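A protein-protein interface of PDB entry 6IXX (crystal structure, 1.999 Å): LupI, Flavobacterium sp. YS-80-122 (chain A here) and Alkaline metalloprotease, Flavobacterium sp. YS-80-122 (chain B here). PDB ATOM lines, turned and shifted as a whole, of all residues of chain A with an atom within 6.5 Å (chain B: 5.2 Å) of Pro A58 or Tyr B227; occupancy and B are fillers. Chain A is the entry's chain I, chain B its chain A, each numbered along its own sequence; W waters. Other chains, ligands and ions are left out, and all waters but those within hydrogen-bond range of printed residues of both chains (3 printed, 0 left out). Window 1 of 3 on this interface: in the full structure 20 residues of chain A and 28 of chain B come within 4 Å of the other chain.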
ATOM      1  N   SER A   1      14.710  -8.065 -10.184  1.00  0.00           N
ATOM      2  CA  SER A   1      13.514  -8.871  -9.905  1.00  0.00           C
ATOM      3  C   SER A   1      13.467  -9.439  -8.487  1.00  0.00           C
ATOM      4  O   SER A   1      14.404 -10.055  -8.032  1.00  0.00           O
ATOM      5  CB  SER A   1      13.378 -10.023 -10.916  1.00  0.00           C
ATOM      6  OG  SER A   1      13.302  -9.571 -12.257  1.00  0.00           O
ATOM      7  N   LEU A   2      12.344  -9.237  -7.805  1.00  0.00           N
ATOM      8  CA  LEU A   2      12.173  -9.798  -6.474  1.00  0.00           C
ATOM      9  C   LEU A   2      12.077 -11.323  -6.534  1.00  0.00           C
ATOM     10  O   LEU A   2      11.566 -11.900  -7.502  1.00  0.00           O
ATOM     11  CB  LEU A   2      10.922  -9.215  -5.819  1.00  0.00           C
ATOM     12  CG  LEU A   2      10.992  -7.700  -5.596  1.00  0.00           C
ATOM     13  CD1 LEU A   2       9.599  -7.103  -5.318  1.00  0.00           C
ATOM     14  CD2 LEU A   2      11.960  -7.399  -4.464  1.00  0.00           C
ATOM     15  N   MET A   3      12.587 -11.975  -5.488  1.00  0.00           N
ATOM     16  CA  MET A   3      12.467 -13.420  -5.340  1.00  0.00           C
ATOM     17  C   MET A   3      11.102 -13.771  -4.756  1.00  0.00           C
ATOM     18  O   MET A   3      10.779 -13.358  -3.635  1.00  0.00           O
ATOM     19  CB  MET A   3      13.582 -13.950  -4.448  1.00  0.00           C
ATOM     20  CG  MET A   3      14.956 -13.877  -5.088  1.00  0.00           C
ATOM     21  SD  MET A   3      16.238 -14.537  -4.016  1.00  0.00           S
ATOM     22  CE  MET A   3      15.716 -16.244  -3.885  1.00  0.00           C
ATOM     23  N   LEU A   4      10.307 -14.537  -5.510  1.00  0.00           N
ATOM     24  CA  LEU A   4       8.969 -14.927  -5.076  1.00  0.00           C
ATOM     25  C   LEU A   4       9.051 -16.082  -4.086  1.00  0.00           C
ATOM     26  O   LEU A   4       9.654 -17.121  -4.376  1.00  0.00           O
ATOM     27  CB  LEU A   4       8.113 -15.326  -6.277  1.00  0.00           C
ATOM     28  CG  LEU A   4       6.811 -16.087  -6.028  1.00  0.00           C
ATOM     29  CD1 LEU A   4       5.814 -15.226  -5.236  1.00  0.00           C
ATOM     30  CD2 LEU A   4       6.225 -16.501  -7.355  1.00  0.00           C
ATOM     31  N   LEU A   5       8.449 -15.901  -2.918  1.00  0.00           N
ATOM     32  CA  LEU A   5       8.509 -16.919  -1.883  1.00  0.00           C
ATOM     33  C   LEU A   5       7.532 -18.041  -2.202  1.00  0.00           C
ATOM     34  O   LEU A   5       6.400 -17.787  -2.619  1.00  0.00           O
ATOM     35  CB  LEU A   5       8.193 -16.300  -0.522  1.00  0.00           C
ATOM     36  CG  LEU A   5       9.323 -15.449   0.065  1.00  0.00           C
ATOM     37  CD1 LEU A   5       8.815 -14.692   1.275  1.00  0.00           C
ATOM     38  CD2 LEU A   5      10.531 -16.303   0.429  1.00  0.00           C
ATOM     39  N   SER A  55      -2.014 -16.197  -1.263  1.00  0.00           N
ATOM     40  CA  SER A  55      -1.119 -16.393  -2.393  1.00  0.00           C
ATOM     41  C   SER A  55       0.060 -15.435  -2.262  1.00  0.00           C
ATOM     42  O   SER A  55      -0.136 -14.221  -2.114  1.00  0.00           O
ATOM     43  CB  SER A  55      -1.863 -16.176  -3.715  1.00  0.00           C
ATOM     44  OG  SER A  55      -1.028 -16.413  -4.835  1.00  0.00           O
ATOM     45  N   PRO A  56       1.294 -15.930  -2.283  1.00  0.00           N
ATOM     46  CA  PRO A  56       2.442 -15.018  -2.221  1.00  0.00           C
ATOM     47  C   PRO A  56       2.581 -14.251  -3.523  1.00  0.00           C
ATOM     48  O   PRO A  56       2.257 -14.755  -4.597  1.00  0.00           O
ATOM     49  CB  PRO A  56       3.637 -15.953  -1.992  1.00  0.00           C
ATOM     50  CG  PRO A  56       3.201 -17.288  -2.492  1.00  0.00           C
ATOM     51  CD  PRO A  56       1.695 -17.347  -2.339  1.00  0.00           C
ATOM     52  N   THR A  57       3.025 -13.005  -3.414  1.00  0.00           N
ATOM     53  CA  THR A  57       3.437 -12.221  -4.562  1.00  0.00           C
ATOM     54  C   THR A  57       4.920 -11.926  -4.382  1.00  0.00           C
ATOM     55  O   THR A  57       5.457 -12.126  -3.287  1.00  0.00           O
ATOM     56  CB  THR A  57       2.628 -10.915  -4.687  1.00  0.00           C
ATOM     57  OG1 THR A  57       3.084  -9.970  -3.719  1.00  0.00           O
ATOM     58  CG2 THR A  57       1.149 -11.171  -4.459  1.00  0.00           C
ATOM     59  N   PRO A  58       5.632 -11.493  -5.430  1.00  0.00           N
ATOM     60  CA  PRO A  58       7.068 -11.211  -5.228  1.00  0.00           C
ATOM     61  C   PRO A  58       7.320 -10.166  -4.155  1.00  0.00           C
ATOM     62  O   PRO A  58       8.341 -10.242  -3.455  1.00  0.00           O
ATOM     63  CB  PRO A  58       7.538 -10.736  -6.610  1.00  0.00           C
ATOM     64  CG  PRO A  58       6.577 -11.383  -7.564  1.00  0.00           C
ATOM     65  CD  PRO A  58       5.245 -11.382  -6.849  1.00  0.00           C
ATOM     66  N   ASP A  59       6.399  -9.212  -3.998  1.00  0.00           N
ATOM     67  CA  ASP A  59       6.534  -8.076  -3.099  1.00  0.00           C
ATOM     68  C   ASP A  59       5.627  -8.162  -1.878  1.00  0.00           C
ATOM     69  O   ASP A  59       5.625  -7.238  -1.055  1.00  0.00           O
ATOM     70  CB  ASP A  59       6.244  -6.771  -3.855  1.00  0.00           C
ATOM     71  CG  ASP A  59       4.795  -6.684  -4.369  1.00  0.00           C
ATOM     72  OD1 ASP A  59       4.249  -7.726  -4.794  1.00  0.00           O
ATOM     73  OD2 ASP A  59       4.204  -5.572  -4.356  1.00  0.00           O
ATOM     74  N   GLY A  60       4.846  -9.229  -1.735  1.00  0.00           N
ATOM     75  CA  GLY A  60       3.946  -9.274  -0.601  1.00  0.00           C
ATOM     76  C   GLY A  60       3.125 -10.541  -0.543  1.00  0.00           C
ATOM     77  O   GLY A  60       3.629 -11.628  -0.843  1.00  0.00           O
ATOM     78  N   LEU A  76       5.431  -7.093   1.783  1.00  0.00           N
ATOM     79  CA  LEU A  76       6.522  -7.644   2.584  1.00  0.00           C
ATOM     80  C   LEU A  76       7.441  -6.514   3.022  1.00  0.00           C
ATOM     81  O   LEU A  76       8.035  -5.830   2.184  1.00  0.00           O
ATOM     82  CB  LEU A  76       7.301  -8.690   1.785  1.00  0.00           C
ATOM     83  CG  LEU A  76       8.500  -9.391   2.447  1.00  0.00           C
ATOM     84  CD1 LEU A  76       8.106 -10.217   3.670  1.00  0.00           C
ATOM     85  CD2 LEU A  76       9.202 -10.258   1.429  1.00  0.00           C
ATOM     86  N   GLY B 160       1.176 -16.621 -17.820  1.00  0.00           N
ATOM     87  CA  GLY B 160       0.536 -16.147 -16.613  1.00  0.00           C
ATOM     88  C   GLY B 160       1.348 -16.246 -15.336  1.00  0.00           C
ATOM     89  O   GLY B 160       0.893 -15.741 -14.301  1.00  0.00           O
ATOM     90  N   ASN B 161       2.519 -16.882 -15.341  1.00  0.00           N
ATOM     91  CA  ASN B 161       3.228 -17.030 -14.078  1.00  0.00           C
ATOM     92  C   ASN B 161       4.454 -16.118 -14.016  1.00  0.00           C
ATOM     93  O   ASN B 161       4.838 -15.456 -14.989  1.00  0.00           O
ATOM     94  CB  ASN B 161       3.565 -18.511 -13.780  1.00  0.00           C
ATOM     95  CG  ASN B 161       4.768 -19.070 -14.558  1.00  0.00           C
ATOM     96  OD1 ASN B 161       5.691 -18.360 -14.958  1.00  0.00           O
ATOM     97  ND2 ASN B 161       4.769 -20.387 -14.713  1.00  0.00           N
ATOM     98  N   TYR B 162       5.043 -16.063 -12.819  1.00  0.00           N
ATOM     99  CA  TYR B 162       6.088 -15.083 -12.552  1.00  0.00           C
ATOM    100  C   TYR B 162       7.386 -15.444 -13.261  1.00  0.00           C
ATOM    101  O   TYR B 162       8.159 -14.551 -13.626  1.00  0.00           O
ATOM    102  CB  TYR B 162       6.309 -14.947 -11.042  1.00  0.00           C
ATOM    103  CG  TYR B 162       7.316 -13.878 -10.660  1.00  0.00           C
ATOM    104  CD1 TYR B 162       7.178 -12.564 -11.109  1.00  0.00           C
ATOM    105  CD2 TYR B 162       8.409 -14.183  -9.852  1.00  0.00           C
ATOM    106  CE1 TYR B 162       8.100 -11.581 -10.758  1.00  0.00           C
ATOM    107  CE2 TYR B 162       9.340 -13.210  -9.500  1.00  0.00           C
ATOM    108  CZ  TYR B 162       9.179 -11.914  -9.954  1.00  0.00           C
ATOM    109  OH  TYR B 162      10.115 -10.965  -9.596  1.00  0.00           O
ATOM    110  N   GLN B 165       7.012 -13.861 -16.678  1.00  0.00           N
ATOM    111  CA  GLN B 165       7.104 -12.405 -16.623  1.00  0.00           C
ATOM    112  C   GLN B 165       8.532 -11.968 -16.348  1.00  0.00           C
ATOM    113  O   GLN B 165       8.964 -10.911 -16.825  1.00  0.00           O
ATOM    114  CB  GLN B 165       6.161 -11.825 -15.563  1.00  0.00           C
ATOM    115  CG  GLN B 165       6.148 -10.278 -15.580  1.00  0.00           C
ATOM    116  CD  GLN B 165       5.182  -9.657 -14.590  1.00  0.00           C
ATOM    117  OE1 GLN B 165       5.534  -9.421 -13.429  1.00  0.00           O
ATOM    118  NE2 GLN B 165       3.967  -9.346 -15.051  1.00  0.00           N
ATOM    119  N   ARG B 202       2.226  -3.598 -11.341  1.00  0.00           N
ATOM    120  CA  ARG B 202       2.145  -4.659 -12.336  1.00  0.00           C
ATOM    121  C   ARG B 202       0.873  -4.599 -13.193  1.00  0.00           C
ATOM    122  O   ARG B 202       0.716  -5.445 -14.082  1.00  0.00           O
ATOM    123  CB  ARG B 202       2.245  -6.012 -11.627  1.00  0.00           C
ATOM    124  CG  ARG B 202       3.663  -6.386 -11.260  1.00  0.00           C
ATOM    125  CD  ARG B 202       3.790  -7.797 -10.627  1.00  0.00           C
ATOM    126  NE  ARG B 202       4.826  -7.761  -9.588  1.00  0.00           N
ATOM    127  CZ  ARG B 202       6.130  -7.949  -9.805  1.00  0.00           C
ATOM    128  NH1 ARG B 202       6.579  -8.240 -11.026  1.00  0.00           N
ATOM    129  NH2 ARG B 202       6.991  -7.858  -8.787  1.00  0.00           N
ATOM    130  N   GLY B 225      -3.500 -15.330  -8.014  1.00  0.00           N
ATOM    131  CA  GLY B 225      -3.291 -14.264  -8.971  1.00  0.00           C
ATOM    132  C   GLY B 225      -2.530 -14.733 -10.205  1.00  0.00           C
ATOM    133  O   GLY B 225      -2.144 -15.892 -10.332  1.00  0.00           O
ATOM    134  N   ALA B 226      -2.335 -13.802 -11.141  1.00  0.00           N
ATOM    135  CA  ALA B 226      -1.536 -14.060 -12.331  1.00  0.00           C
ATOM    136  C   ALA B 226      -0.680 -12.840 -12.645  1.00  0.00           C
ATOM    137  O   ALA B 226      -0.850 -11.768 -12.062  1.00  0.00           O
ATOM    138  CB  ALA B 226      -2.407 -14.420 -13.539  1.00  0.00           C
ATOM    139  N   TYR B 227       0.223 -13.022 -13.610  1.00  0.00           N
ATOM    140  CA  TYR B 227       1.213 -12.036 -14.017  1.00  0.00           C
ATOM    141  C   TYR B 227       1.200 -11.938 -15.532  1.00  0.00           C
ATOM    142  O   TYR B 227       1.279 -12.963 -16.213  1.00  0.00           O
ATOM    143  CB  TYR B 227       2.627 -12.424 -13.530  1.00  0.00           C
ATOM    144  CG  TYR B 227       2.693 -12.684 -12.039  1.00  0.00           C
ATOM    145  CD1 TYR B 227       2.976 -11.653 -11.149  1.00  0.00           C
ATOM    146  CD2 TYR B 227       2.425 -13.947 -11.519  1.00  0.00           C
ATOM    147  CE1 TYR B 227       3.015 -11.877  -9.789  1.00  0.00           C
ATOM    148  CE2 TYR B 227       2.453 -14.182 -10.152  1.00  0.00           C
ATOM    149  CZ  TYR B 227       2.755 -13.143  -9.298  1.00  0.00           C
ATOM    150  OH  TYR B 227       2.783 -13.371  -7.949  1.00  0.00           O
ATOM    151  N   ALA B 228       1.116 -10.714 -16.053  1.00  0.00           N
ATOM    152  CA  ALA B 228       1.209 -10.492 -17.493  1.00  0.00           C
ATOM    153  C   ALA B 228       2.483 -11.105 -18.071  1.00  0.00           C
ATOM    154  O   ALA B 228       3.589 -10.854 -17.583  1.00  0.00           O
ATOM    155  CB  ALA B 228       1.175  -8.989 -17.788  1.00  0.00           C
ATOM    156  N   SER B 229       2.325 -11.903 -19.128  1.00  0.00           N
ATOM    157  CA  SER B 229       3.479 -12.515 -19.781  1.00  0.00           C
ATOM    158  C   SER B 229       4.146 -11.602 -20.798  1.00  0.00           C
ATOM    159  O   SER B 229       5.317 -11.826 -21.134  1.00  0.00           O
ATOM    160  CB  SER B 229       3.069 -13.827 -20.462  1.00  0.00           C
ATOM    161  OG  SER B 229       2.576 -14.768 -19.522  1.00  0.00           O
ATOM    162  N   ILE B 277      -4.476 -11.210 -18.805  1.00  0.00           N
ATOM    163  CA  ILE B 277      -3.825  -9.941 -18.497  1.00  0.00           C
ATOM    164  C   ILE B 277      -3.016  -9.563 -19.726  1.00  0.00           C
ATOM    165  O   ILE B 277      -1.994 -10.198 -20.007  1.00  0.00           O
ATOM    166  CB  ILE B 277      -2.900 -10.011 -17.273  1.00  0.00           C
ATOM    167  CG1 ILE B 277      -3.580 -10.658 -16.071  1.00  0.00           C
ATOM    168  CG2 ILE B 277      -2.427  -8.613 -16.910  1.00  0.00           C
ATOM    169  CD1 ILE B 277      -2.595 -11.107 -15.008  1.00  0.00           C
HETATM  170  O   HOH W   1      10.714 -10.091 -12.747  1.00  0.00           O
HETATM  171  O   HOH W   2       3.183  -8.263  -7.308  1.00  0.00           O
HETATM  172  O   HOH W   3       9.931  -8.333  -9.233  1.00  0.00           O
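Among the printed residues, merely in contact across the chains: Ser A1 with Tyr B162 (3.6 Å), Leu A4 with Tyr B162 (3.8 Å), Pro A56 with Tyr B227 (3.7 Å), Thr A57 with Tyr B227 (3.6 Å), Pro A58 with Tyr B162 (3.5 Å), Pro A58 with Arg B202 (3.6 Å) and Pro A58 with Tyr B227 (3.4 Å).
The side-chain hydroxyl of Thr A57 sits at hydrogen-bond distance from the backbone NH of Gly A60 (2.8 Å).
O of Gly B160 sits at hydrogen-bond distance from N of Tyr B227, 2.9 Å away.
OG1 of Thr A57 lies within hydrogen-bond range of OD1 of Asp A59 (2.7 Å).
The guanidinium group (NH1) of Arg B202 lies within hydrogen-bond range of the side-chain amide oxygen (OE1) of Gln B165 (2.9 Å).
Of the 11 printed residues of chain B, 3 touch a printed residue of chain A.
Of the 12 printed residues of chain A, 6 touch a printed residue of chain B.
Hydrophobic or aromatic side chains of chain A that line the printed part of chain B: Leu A4 and Pro A58.
Among the printed residues, 8 pairs touch across the chains.
Among the printed residues, no Asp or Glu carboxylate lies within 4 Å of a Lys or Arg side-chain nitrogen of the other chain.
Printed residues of chain B within 4 Å of Leu A2: Tyr B162.
Printed residues of chain B within 4 Å of Leu A4: Tyr B162 (3.8 Å).
Of the printed residues of chain B, Thr A57 touches Tyr B227.
Of the printed residues of chain B, Pro A58 touches Tyr B162 (3.5 Å), Arg B202 (3.6 Å) and Tyr B227 (3.4 Å).
Gly B160 touches none of the printed residues of chain A.
Printed residues of chain A within 4 Å of Tyr B162: Ser A1 (3.6 Å), Leu A2 (2.7 Å), Leu A4 (3.8 Å) and Pro A58 (3.5 Å).
Tyr B227 touches just these residues of chain A: Pro A56 (3.7 Å), Thr A57 (3.6 Å) and Pro A58 (3.4 Å).
The nearest printed residue of chain B that does not touch Pro A58 is Gln B165 (6.3 Å).
The nearest residue of chain A that does not touch Tyr B227 is Leu A4 (4.5 Å).
Water W3 lies within hydrogen-bond range of OH of Tyr B162, N of Leu A2 and NH2 of Arg B202.
Water W1 bridges OG of Ser A1 (2.7 Å) and OH of Tyr B162 (3.3 Å).
Water W2 bridges OD1 of Asp A59 (2.8 Å) and NE of Arg B202 (2.9 Å).
The side-chain hydroxyl (OH) of Tyr B162 is in hydrogen-bond range of the backbone carbonyl oxygen (O) of Leu A2 (2.7 Å).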
